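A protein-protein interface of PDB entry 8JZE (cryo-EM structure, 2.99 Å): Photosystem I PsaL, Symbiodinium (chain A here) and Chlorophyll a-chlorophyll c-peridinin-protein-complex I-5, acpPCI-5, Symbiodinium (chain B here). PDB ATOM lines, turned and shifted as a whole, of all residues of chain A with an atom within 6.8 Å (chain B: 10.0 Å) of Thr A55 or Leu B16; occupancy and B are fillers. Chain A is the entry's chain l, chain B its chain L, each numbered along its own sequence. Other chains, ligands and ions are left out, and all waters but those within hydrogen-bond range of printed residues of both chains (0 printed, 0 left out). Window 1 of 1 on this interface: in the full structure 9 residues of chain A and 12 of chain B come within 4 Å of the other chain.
The backbone carbonyl oxygen (O) of Met A57 lies within hydrogen-bond range of the backbone NH (N) of Ile B14 (2.8 Å).
The backbone carbonyl oxygen (O) of Leu B16 lies within hydrogen-bond range of the side-chain hydroxyl (OG1) of Thr A11 (3.0 Å).
NZ of Lys A56 is in salt-bridge range of OD2 of Asp B15 (3.5 Å).
The guanidinium group of Arg A10 is in hydrogen-bond range of the side-chain hydroxyl of Thr B47, at 3.2 Å.
NH2 of Arg A10 is in hydrogen-bond range of O of Lys B45, at 2.7 Å.
The backbone carbonyl oxygen (O) of Thr A55 lies within hydrogen-bond range of the backbone NH (N) of Leu B16 (2.8 Å).
OD1 of Asp B15 sits close to O of Thr A55 (3.4 Å).
Leu B16 touches just these residues of chain A: Pro A9, Thr A11, Tyr A49, Thr A55, Met A57 and Tyr A62.
Of chain B, only Leu B16, Thr B47 and Glu B48 come within 4 Å of Thr A11.
No residue of chain B comes within 4 Å of Gly A50.
Ala A54 touches none of the printed residues of chain B.
Printed residues of chain A within 4 Å of Ile B14: Lys A56 (3.7 Å), Met A57 (2.8 Å) and Tyr A62 (3.4 Å).
Of the printed residues of chain A, Asp B11 touches Lys A56.
Printed residues of chain A within 4 Å of Gly B13: Met A57 (3.5 Å).
Printed residues of chain A within 4 Å of Thr B47: Arg A10 and Thr A11.
Printed residues of chain A within 4 Å of Tyr B46: Arg A10 (3.5 Å).
The nearest residue of chain A that does not touch Leu B16 is Ala A54 (4.4 Å).
The side-chain carboxylate (OD1) of Asp B15 sits at hydrogen-bond distance from the backbone NH (N) of Met B17, at 2.9 Å.
O of Thr A11 lies within hydrogen-bond range of OH of Tyr A62, at 3.1 Å.
N of Tyr A62 lies within hydrogen-bond range of SD of Met A57 (3.8 Å).
Among the printed residues, pairs that only touch across the chains: Lys A56 with Asp B11, Tyr A62 with Ile B14, Pro A9 with Leu B16, Arg A10 with Tyr B46, Tyr A62 with Glu B48, Met A57 with Gly B13, Tyr A49 with Leu B16, Tyr A62 with Leu B16, Met A57 with Leu B16, Thr A55 with Met B17, Lys A56 with Ile B14, Thr A11 with Thr B47 and Thr A11 with Glu B48.
Of the 16 printed residues of chain A, 8 touch a printed residue of chain B.
Printed residues of chain A that touch a printed residue of chain B: Pro A9, Arg A10, Thr A11, Tyr A49, Thr A55, Lys A56, Met A57 and Tyr A62.
Among the printed residues, 20 pairs touch across the chains.
Among the printed residues, Asp or Glu carboxylates within 4 Å of a Lys or Arg side-chain nitrogen of the other chain: Lys A56 with Asp B15 (3.5 Å).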
ATOM      1  N   PRO A   9      35.938  -6.943  15.649  1.00  0.00           N
ATOM      2  CA  PRO A   9      35.191  -6.314  16.744  1.00  0.00           C
ATOM      3  C   PRO A   9      34.350  -7.331  17.498  1.00  0.00           C
ATOM      4  O   PRO A   9      33.822  -8.282  16.918  1.00  0.00           O
ATOM      5  CB  PRO A   9      34.315  -5.279  16.029  1.00  0.00           C
ATOM      6  CG  PRO A   9      35.000  -5.029  14.727  1.00  0.00           C
ATOM      7  CD  PRO A   9      35.631  -6.333  14.346  1.00  0.00           C
ATOM      8  N   ARG A  10      34.240  -7.126  18.812  1.00  0.00           N
ATOM      9  CA  ARG A  10      33.396  -7.995  19.625  1.00  0.00           C
ATOM     10  C   ARG A  10      31.936  -7.893  19.205  1.00  0.00           C
ATOM     11  O   ARG A  10      31.185  -8.866  19.329  1.00  0.00           O
ATOM     12  CB  ARG A  10      33.563  -7.648  21.107  1.00  0.00           C
ATOM     13  CG  ARG A  10      32.986  -8.666  22.089  1.00  0.00           C
ATOM     14  CD  ARG A  10      31.542  -8.360  22.440  1.00  0.00           C
ATOM     15  NE  ARG A  10      31.339  -6.936  22.672  1.00  0.00           N
ATOM     16  CZ  ARG A  10      30.152  -6.352  22.747  1.00  0.00           C
ATOM     17  NH1 ARG A  10      29.033  -7.043  22.615  1.00  0.00           N
ATOM     18  NH2 ARG A  10      30.087  -5.040  22.950  1.00  0.00           N
ATOM     19  N   THR A  11      31.520  -6.728  18.701  1.00  0.00           N
ATOM     20  CA  THR A  11      30.136  -6.555  18.273  1.00  0.00           C
ATOM     21  C   THR A  11      29.783  -7.479  17.114  1.00  0.00           C
ATOM     22  O   THR A  11      28.634  -7.920  17.003  1.00  0.00           O
ATOM     23  CB  THR A  11      29.885  -5.098  17.882  1.00  0.00           C
ATOM     24  OG1 THR A  11      30.919  -4.655  16.995  1.00  0.00           O
ATOM     25  CG2 THR A  11      29.869  -4.211  19.117  1.00  0.00           C
ATOM     26  N   ILE A  12      30.745  -7.774  16.237  1.00  0.00           N
ATOM     27  CA  ILE A  12      30.481  -8.694  15.135  1.00  0.00           C
ATOM     28  C   ILE A  12      30.328 -10.117  15.656  1.00  0.00           C
ATOM     29  O   ILE A  12      29.370 -10.821  15.315  1.00  0.00           O
ATOM     30  CB  ILE A  12      31.590  -8.591  14.072  1.00  0.00           C
ATOM     31  CG1 ILE A  12      31.596  -7.194  13.450  1.00  0.00           C
ATOM     32  CG2 ILE A  12      31.406  -9.657  13.003  1.00  0.00           C
ATOM     33  CD1 ILE A  12      32.593  -7.027  12.327  1.00  0.00           C
ATOM     34  N   MET A  48      34.522  -6.358   5.917  1.00  0.00           N
ATOM     35  CA  MET A  48      33.779  -5.141   5.613  1.00  0.00           C
ATOM     36  C   MET A  48      33.648  -4.210   6.803  1.00  0.00           C
ATOM     37  O   MET A  48      33.683  -2.990   6.633  1.00  0.00           O
ATOM     38  CB  MET A  48      32.375  -5.482   5.102  1.00  0.00           C
ATOM     39  CG  MET A  48      32.338  -6.641   4.137  1.00  0.00           C
ATOM     40  SD  MET A  48      33.610  -6.498   2.878  1.00  0.00           S
ATOM     41  CE  MET A  48      33.742  -8.200   2.337  1.00  0.00           C
ATOM     42  N   TYR A  49      33.488  -4.756   8.005  1.00  0.00           N
ATOM     43  CA  TYR A  49      33.296  -3.968   9.214  1.00  0.00           C
ATOM     44  C   TYR A  49      34.443  -4.235  10.174  1.00  0.00           C
ATOM     45  O   TYR A  49      34.784  -5.394  10.435  1.00  0.00           O
ATOM     46  CB  TYR A  49      31.952  -4.294   9.867  1.00  0.00           C
ATOM     47  CG  TYR A  49      30.776  -4.133   8.931  1.00  0.00           C
ATOM     48  CD1 TYR A  49      30.352  -2.874   8.531  1.00  0.00           C
ATOM     49  CD2 TYR A  49      30.090  -5.240   8.446  1.00  0.00           C
ATOM     50  CE1 TYR A  49      29.282  -2.719   7.674  1.00  0.00           C
ATOM     51  CE2 TYR A  49      29.018  -5.096   7.590  1.00  0.00           C
ATOM     52  CZ  TYR A  49      28.619  -3.833   7.207  1.00  0.00           C
ATOM     53  OH  TYR A  49      27.550  -3.682   6.355  1.00  0.00           O
ATOM     54  N   GLY A  50      35.037  -3.164  10.694  1.00  0.00           N
ATOM     55  CA  GLY A  50      36.161  -3.273  11.590  1.00  0.00           C
ATOM     56  C   GLY A  50      36.764  -1.925  11.923  1.00  0.00           C
ATOM     57  O   GLY A  50      36.175  -0.872  11.656  1.00  0.00           O
ATOM     58  N   PRO A  51      37.957  -1.934  12.524  1.00  0.00           N
ATOM     59  CA  PRO A  51      38.585  -0.656  12.909  1.00  0.00           C
ATOM     60  C   PRO A  51      38.913   0.243  11.727  1.00  0.00           C
ATOM     61  O   PRO A  51      38.560   1.428  11.738  1.00  0.00           O
ATOM     62  CB  PRO A  51      39.847  -1.107  13.660  1.00  0.00           C
ATOM     63  CG  PRO A  51      39.543  -2.496  14.120  1.00  0.00           C
ATOM     64  CD  PRO A  51      38.702  -3.095  13.036  1.00  0.00           C
ATOM     65  N   GLY A  52      39.579  -0.286  10.707  1.00  0.00           N
ATOM     66  CA  GLY A  52      39.941   0.487   9.538  1.00  0.00           C
ATOM     67  C   GLY A  52      38.883   0.545   8.460  1.00  0.00           C
ATOM     68  O   GLY A  52      39.136   1.100   7.386  1.00  0.00           O
ATOM     69  N   LYS A  53      37.701  -0.010   8.715  1.00  0.00           N
ATOM     70  CA  LYS A  53      36.651  -0.123   7.712  1.00  0.00           C
ATOM     71  C   LYS A  53      35.357   0.481   8.240  1.00  0.00           C
ATOM     72  O   LYS A  53      35.372   1.202   9.241  1.00  0.00           O
ATOM     73  CB  LYS A  53      36.442  -1.586   7.319  1.00  0.00           C
ATOM     74  CG  LYS A  53      37.733  -2.338   7.042  1.00  0.00           C
ATOM     75  CD  LYS A  53      37.472  -3.803   6.758  1.00  0.00           C
ATOM     76  CE  LYS A  53      38.762  -4.607   6.794  1.00  0.00           C
ATOM     77  NZ  LYS A  53      39.409  -4.544   8.134  1.00  0.00           N
ATOM     78  N   ALA A  54      34.242   0.218   7.555  1.00  0.00           N
ATOM     79  CA  ALA A  54      32.934   0.690   7.994  1.00  0.00           C
ATOM     80  C   ALA A  54      32.674   0.307   9.446  1.00  0.00           C
ATOM     81  O   ALA A  54      32.547  -0.877   9.770  1.00  0.00           O
ATOM     82  CB  ALA A  54      31.835   0.122   7.095  1.00  0.00           C
ATOM     83  N   THR A  55      32.592   1.304  10.322  1.00  0.00           N
ATOM     84  CA  THR A  55      32.432   1.081  11.753  1.00  0.00           C
ATOM     85  C   THR A  55      30.979   1.116  12.207  1.00  0.00           C
ATOM     86  O   THR A  55      30.719   0.955  13.404  1.00  0.00           O
ATOM     87  CB  THR A  55      33.232   2.123  12.541  1.00  0.00           C
ATOM     88  OG1 THR A  55      32.815   3.438  12.157  1.00  0.00           O
ATOM     89  CG2 THR A  55      34.720   1.972  12.275  1.00  0.00           C
ATOM     90  N   LYS A  56      30.033   1.323  11.297  1.00  0.00           N
ATOM     91  CA  LYS A  56      28.626   1.413  11.655  1.00  0.00           C
ATOM     92  C   LYS A  56      27.801   0.588  10.681  1.00  0.00           C
ATOM     93  O   LYS A  56      28.210   0.333   9.546  1.00  0.00           O
ATOM     94  CB  LYS A  56      28.138   2.869  11.672  1.00  0.00           C
ATOM     95  CG  LYS A  56      28.686   3.690  12.825  1.00  0.00           C
ATOM     96  CD  LYS A  56      28.289   5.150  12.711  1.00  0.00           C
ATOM     97  CE  LYS A  56      28.795   5.942  13.903  1.00  0.00           C
ATOM     98  NZ  LYS A  56      30.242   5.693  14.157  1.00  0.00           N
ATOM     99  N   MET A  57      26.634   0.158  11.149  1.00  0.00           N
ATOM    100  CA  MET A  57      25.695  -0.594  10.332  1.00  0.00           C
ATOM    101  C   MET A  57      24.288  -0.092  10.607  1.00  0.00           C
ATOM    102  O   MET A  57      23.994   0.434  11.682  1.00  0.00           O
ATOM    103  CB  MET A  57      25.765  -2.099  10.618  1.00  0.00           C
ATOM    104  CG  MET A  57      26.215  -2.937   9.442  1.00  0.00           C
ATOM    105  SD  MET A  57      26.047  -4.705   9.751  1.00  0.00           S
ATOM    106  CE  MET A  57      26.880  -4.852  11.327  1.00  0.00           C
ATOM    107  N   TYR A  62      22.515  -5.057  11.073  1.00  0.00           N
ATOM    108  CA  TYR A  62      23.136  -5.645  12.255  1.00  0.00           C
ATOM    109  C   TYR A  62      22.246  -6.719  12.866  1.00  0.00           C
ATOM    110  O   TYR A  62      22.744  -7.732  13.369  1.00  0.00           O
ATOM    111  CB  TYR A  62      23.454  -4.565  13.287  1.00  0.00           C
ATOM    112  CG  TYR A  62      24.135  -5.101  14.527  1.00  0.00           C
ATOM    113  CD1 TYR A  62      25.502  -5.348  14.538  1.00  0.00           C
ATOM    114  CD2 TYR A  62      23.414  -5.358  15.686  1.00  0.00           C
ATOM    115  CE1 TYR A  62      26.129  -5.836  15.663  1.00  0.00           C
ATOM    116  CE2 TYR A  62      24.034  -5.845  16.818  1.00  0.00           C
ATOM    117  CZ  TYR A  62      25.391  -6.083  16.799  1.00  0.00           C
ATOM    118  OH  TYR A  62      26.015  -6.570  17.924  1.00  0.00           O
ATOM    119  N   LEU A  65      22.722  -9.745  10.764  1.00  0.00           N
ATOM    120  CA  LEU A  65      24.039 -10.312  11.033  1.00  0.00           C
ATOM    121  C   LEU A  65      24.040 -11.099  12.336  1.00  0.00           C
ATOM    122  O   LEU A  65      24.600 -12.197  12.407  1.00  0.00           O
ATOM    123  CB  LEU A  65      25.095  -9.206  11.077  1.00  0.00           C
ATOM    124  CG  LEU A  65      26.484  -9.632  11.563  1.00  0.00           C
ATOM    125  CD1 LEU A  65      27.081 -10.675  10.638  1.00  0.00           C
ATOM    126  CD2 LEU A  65      27.414  -8.439  11.690  1.00  0.00           C
ATOM    127  N   GLU B  10      23.385  11.853  10.974  1.00  0.00           N
ATOM    128  CA  GLU B  10      24.372  11.376  10.014  1.00  0.00           C
ATOM    129  C   GLU B  10      25.398  10.436  10.636  1.00  0.00           C
ATOM    130  O   GLU B  10      26.137   9.783   9.893  1.00  0.00           O
ATOM    131  CB  GLU B  10      25.082  12.561   9.356  1.00  0.00           C
ATOM    132  CG  GLU B  10      24.180  13.397   8.460  1.00  0.00           C
ATOM    133  CD  GLU B  10      24.948  14.411   7.636  1.00  0.00           C
ATOM    134  OE1 GLU B  10      25.988  14.909   8.116  1.00  0.00           O
ATOM    135  OE2 GLU B  10      24.515  14.707   6.504  1.00  0.00           O
ATOM    136  N   ASP B  11      25.461  10.352  11.964  1.00  0.00           N
ATOM    137  CA  ASP B  11      26.351   9.426  12.654  1.00  0.00           C
ATOM    138  C   ASP B  11      25.567   8.400  13.467  1.00  0.00           C
ATOM    139  O   ASP B  11      26.060   7.887  14.474  1.00  0.00           O
ATOM    140  CB  ASP B  11      27.334  10.177  13.552  1.00  0.00           C
ATOM    141  CG  ASP B  11      28.383  10.940  12.765  1.00  0.00           C
ATOM    142  OD1 ASP B  11      28.209  11.104  11.540  1.00  0.00           O
ATOM    143  OD2 ASP B  11      29.387  11.366  13.373  1.00  0.00           O
ATOM    144  N   ALA B  12      24.347   8.091  13.041  1.00  0.00           N
ATOM    145  CA  ALA B  12      23.494   7.134  13.728  1.00  0.00           C
ATOM    146  C   ALA B  12      23.680   5.736  13.145  1.00  0.00           C
ATOM    147  O   ALA B  12      24.270   5.548  12.079  1.00  0.00           O
ATOM    148  CB  ALA B  12      22.027   7.563  13.643  1.00  0.00           C
ATOM    149  N   GLY B  13      23.166   4.748  13.869  1.00  0.00           N
ATOM    150  CA  GLY B  13      23.279   3.356  13.499  1.00  0.00           C
ATOM    151  C   GLY B  13      23.897   2.536  14.609  1.00  0.00           C
ATOM    152  O   GLY B  13      24.300   3.046  15.652  1.00  0.00           O
ATOM    153  N   ILE B  14      23.971   1.229  14.364  1.00  0.00           N
ATOM    154  CA  ILE B  14      24.542   0.292  15.330  1.00  0.00           C
ATOM    155  C   ILE B  14      26.060   0.437  15.257  1.00  0.00           C
ATOM    156  O   ILE B  14      26.704  -0.111  14.361  1.00  0.00           O
ATOM    157  CB  ILE B  14      24.101  -1.148  15.066  1.00  0.00           C
ATOM    158  CG1 ILE B  14      22.577  -1.271  15.148  1.00  0.00           C
ATOM    159  CG2 ILE B  14      24.763  -2.088  16.059  1.00  0.00           C
ATOM    160  CD1 ILE B  14      22.017  -1.076  16.537  1.00  0.00           C
ATOM    161  N   ASP B  15      26.637   1.184  16.196  1.00  0.00           N
ATOM    162  CA  ASP B  15      28.080   1.369  16.217  1.00  0.00           C
ATOM    163  C   ASP B  15      28.773   0.052  16.541  1.00  0.00           C
ATOM    164  O   ASP B  15      28.391  -0.652  17.479  1.00  0.00           O
ATOM    165  CB  ASP B  15      28.460   2.440  17.241  1.00  0.00           C
ATOM    166  CG  ASP B  15      29.846   3.017  17.001  1.00  0.00           C
ATOM    167  OD1 ASP B  15      30.730   2.285  16.509  1.00  0.00           O
ATOM    168  OD2 ASP B  15      30.047   4.213  17.302  1.00  0.00           O
ATOM    169  N   LEU B  16      29.798  -0.277  15.756  1.00  0.00           N
ATOM    170  CA  LEU B  16      30.537  -1.524  15.903  1.00  0.00           C
ATOM    171  C   LEU B  16      31.873  -1.328  16.608  1.00  0.00           C
ATOM    172  O   LEU B  16      32.700  -2.246  16.623  1.00  0.00           O
ATOM    173  CB  LEU B  16      30.748  -2.171  14.535  1.00  0.00           C
ATOM    174  CG  LEU B  16      29.468  -2.531  13.783  1.00  0.00           C
ATOM    175  CD1 LEU B  16      29.786  -3.000  12.382  1.00  0.00           C
ATOM    176  CD2 LEU B  16      28.698  -3.595  14.536  1.00  0.00           C
ATOM    177  N   MET B  17      32.102  -0.154  17.190  1.00  0.00           N
ATOM    178  CA  MET B  17      33.351   0.156  17.866  1.00  0.00           C
ATOM    179  C   MET B  17      33.067   0.523  19.316  1.00  0.00           C
ATOM    180  O   MET B  17      31.917   0.706  19.724  1.00  0.00           O
ATOM    181  CB  MET B  17      34.102   1.291  17.159  1.00  0.00           C
ATOM    182  CG  MET B  17      34.556   0.938  15.754  1.00  0.00           C
ATOM    183  SD  MET B  17      35.492  -0.602  15.695  1.00  0.00           S
ATOM    184  CE  MET B  17      36.850  -0.217  16.796  1.00  0.00           C
ATOM    185  N   ASP B  18      34.138   0.629  20.098  1.00  0.00           N
ATOM    186  CA  ASP B  18      34.051   0.884  21.528  1.00  0.00           C
ATOM    187  C   ASP B  18      34.691   2.229  21.845  1.00  0.00           C
ATOM    188  O   ASP B  18      35.843   2.476  21.471  1.00  0.00           O
ATOM    189  CB  ASP B  18      34.737  -0.231  22.321  1.00  0.00           C
ATOM    190  CG  ASP B  18      34.231  -0.333  23.747  1.00  0.00           C
ATOM    191  OD1 ASP B  18      33.699   0.670  24.269  1.00  0.00           O
ATOM    192  OD2 ASP B  18      34.366  -1.419  24.345  1.00  0.00           O
ATOM    193  N   ASN B  19      33.942   3.092  22.534  1.00  0.00           N
ATOM    194  CA  ASN B  19      34.486   4.384  22.940  1.00  0.00           C
ATOM    195  C   ASN B  19      35.588   4.220  23.977  1.00  0.00           C
ATOM    196  O   ASN B  19      36.529   5.020  24.025  1.00  0.00           O
ATOM    197  CB  ASN B  19      33.375   5.280  23.488  1.00  0.00           C
ATOM    198  CG  ASN B  19      32.522   5.893  22.396  1.00  0.00           C
ATOM    199  OD1 ASN B  19      32.454   5.379  21.280  1.00  0.00           O
ATOM    200  ND2 ASN B  19      31.865   7.003  22.713  1.00  0.00           N
ATOM    201  N   GLN B  24      29.863   3.813  26.798  1.00  0.00           N
ATOM    202  CA  GLN B  24      30.087   4.597  25.588  1.00  0.00           C
ATOM    203  C   GLN B  24      29.960   6.098  25.821  1.00  0.00           C
ATOM    204  O   GLN B  24      29.401   6.815  24.985  1.00  0.00           O
ATOM    205  CB  GLN B  24      29.128   4.144  24.490  1.00  0.00           C
ATOM    206  CG  GLN B  24      29.243   2.663  24.177  1.00  0.00           C
ATOM    207  CD  GLN B  24      30.683   2.184  24.182  1.00  0.00           C
ATOM    208  OE1 GLN B  24      31.457   2.496  23.277  1.00  0.00           O
ATOM    209  NE2 GLN B  24      31.052   1.430  25.211  1.00  0.00           N
ATOM    210  N   LYS B  45      28.631  -3.729  28.769  1.00  0.00           N
ATOM    211  CA  LYS B  45      29.703  -4.326  27.982  1.00  0.00           C
ATOM    212  C   LYS B  45      29.231  -4.712  26.589  1.00  0.00           C
ATOM    213  O   LYS B  45      30.048  -4.771  25.664  1.00  0.00           O
ATOM    214  CB  LYS B  45      30.276  -5.549  28.697  1.00  0.00           C
ATOM    215  CG  LYS B  45      30.940  -5.244  30.030  1.00  0.00           C
ATOM    216  CD  LYS B  45      31.558  -6.499  30.629  1.00  0.00           C
ATOM    217  CE  LYS B  45      32.078  -6.256  32.037  1.00  0.00           C
ATOM    218  NZ  LYS B  45      32.630  -7.502  32.643  1.00  0.00           N
ATOM    219  N   TYR B  46      27.935  -4.980  26.421  1.00  0.00           N
ATOM    220  CA  TYR B  46      27.334  -5.138  25.097  1.00  0.00           C
ATOM    221  C   TYR B  46      27.112  -3.743  24.511  1.00  0.00           C
ATOM    222  O   TYR B  46      26.002  -3.209  24.468  1.00  0.00           O
ATOM    223  CB  TYR B  46      26.040  -5.933  25.184  1.00  0.00           C
ATOM    224  N   THR B  47      28.220  -3.150  24.058  1.00  0.00           N
ATOM    225  CA  THR B  47      28.228  -1.745  23.666  1.00  0.00           C
ATOM    226  C   THR B  47      27.280  -1.463  22.508  1.00  0.00           C
ATOM    227  O   THR B  47      26.801  -0.334  22.362  1.00  0.00           O
ATOM    228  CB  THR B  47      29.648  -1.319  23.298  1.00  0.00           C
ATOM    229  OG1 THR B  47      30.048  -1.980  22.091  1.00  0.00           O
ATOM    230  CG2 THR B  47      30.611  -1.700  24.407  1.00  0.00           C
ATOM    231  N   GLU B  48      27.000  -2.470  21.677  1.00  0.00           N
ATOM    232  CA  GLU B  48      26.096  -2.272  20.550  1.00  0.00           C
ATOM    233  C   GLU B  48      24.690  -1.892  20.994  1.00  0.00           C
ATOM    234  O   GLU B  48      23.948  -1.289  20.212  1.00  0.00           O
ATOM    235  CB  GLU B  48      26.045  -3.536  19.690  1.00  0.00           C
ATOM    236  N   LEU B  49      24.310  -2.222  22.227  1.00  0.00           N
ATOM    237  CA  LEU B  49      22.968  -1.964  22.732  1.00  0.00           C
ATOM    238  C   LEU B  49      22.905  -0.794  23.705  1.00  0.00           C
ATOM    239  O   LEU B  49      21.823  -0.498  24.221  1.00  0.00           O
ATOM    240  CB  LEU B  49      22.414  -3.223  23.406  1.00  0.00           C
ATOM    241  CG  LEU B  49      22.273  -4.474  22.537  1.00  0.00           C
ATOM    242  CD1 LEU B  49      21.891  -5.679  23.378  1.00  0.00           C
ATOM    243  CD2 LEU B  49      21.249  -4.249  21.441  1.00  0.00           C
ATOM    244  N   PRO B  51      23.084   2.566  23.240  1.00  0.00           N
ATOM    245  CA  PRO B  51      22.059   3.548  22.848  1.00  0.00           C
ATOM    246  C   PRO B  51      20.644   3.043  23.061  1.00  0.00           C
ATOM    247  O   PRO B  51      19.762   3.820  23.446  1.00  0.00           O
ATOM    248  CB  PRO B  51      22.358   3.792  21.363  1.00  0.00           C
ATOM    249  CG  PRO B  51      23.790   3.465  21.212  1.00  0.00           C
ATOM    250  CD  PRO B  51      24.042   2.323  22.146  1.00  0.00           C
ATOM    251  N   VAL B 130      24.433   6.674  20.147  1.00  0.00           N
ATOM    252  CA  VAL B 130      24.864   7.013  21.501  1.00  0.00           C
ATOM    253  C   VAL B 130      24.807   8.508  21.761  1.00  0.00           C
ATOM    254  O   VAL B 130      25.061   8.946  22.890  1.00  0.00           O
ATOM    255  CB  VAL B 130      26.286   6.467  21.744  1.00  0.00           C
ATOM    256  CG1 VAL B 130      27.327   7.393  21.134  1.00  0.00           C
ATOM    257  CG2 VAL B 130      26.537   6.244  23.225  1.00  0.00           C
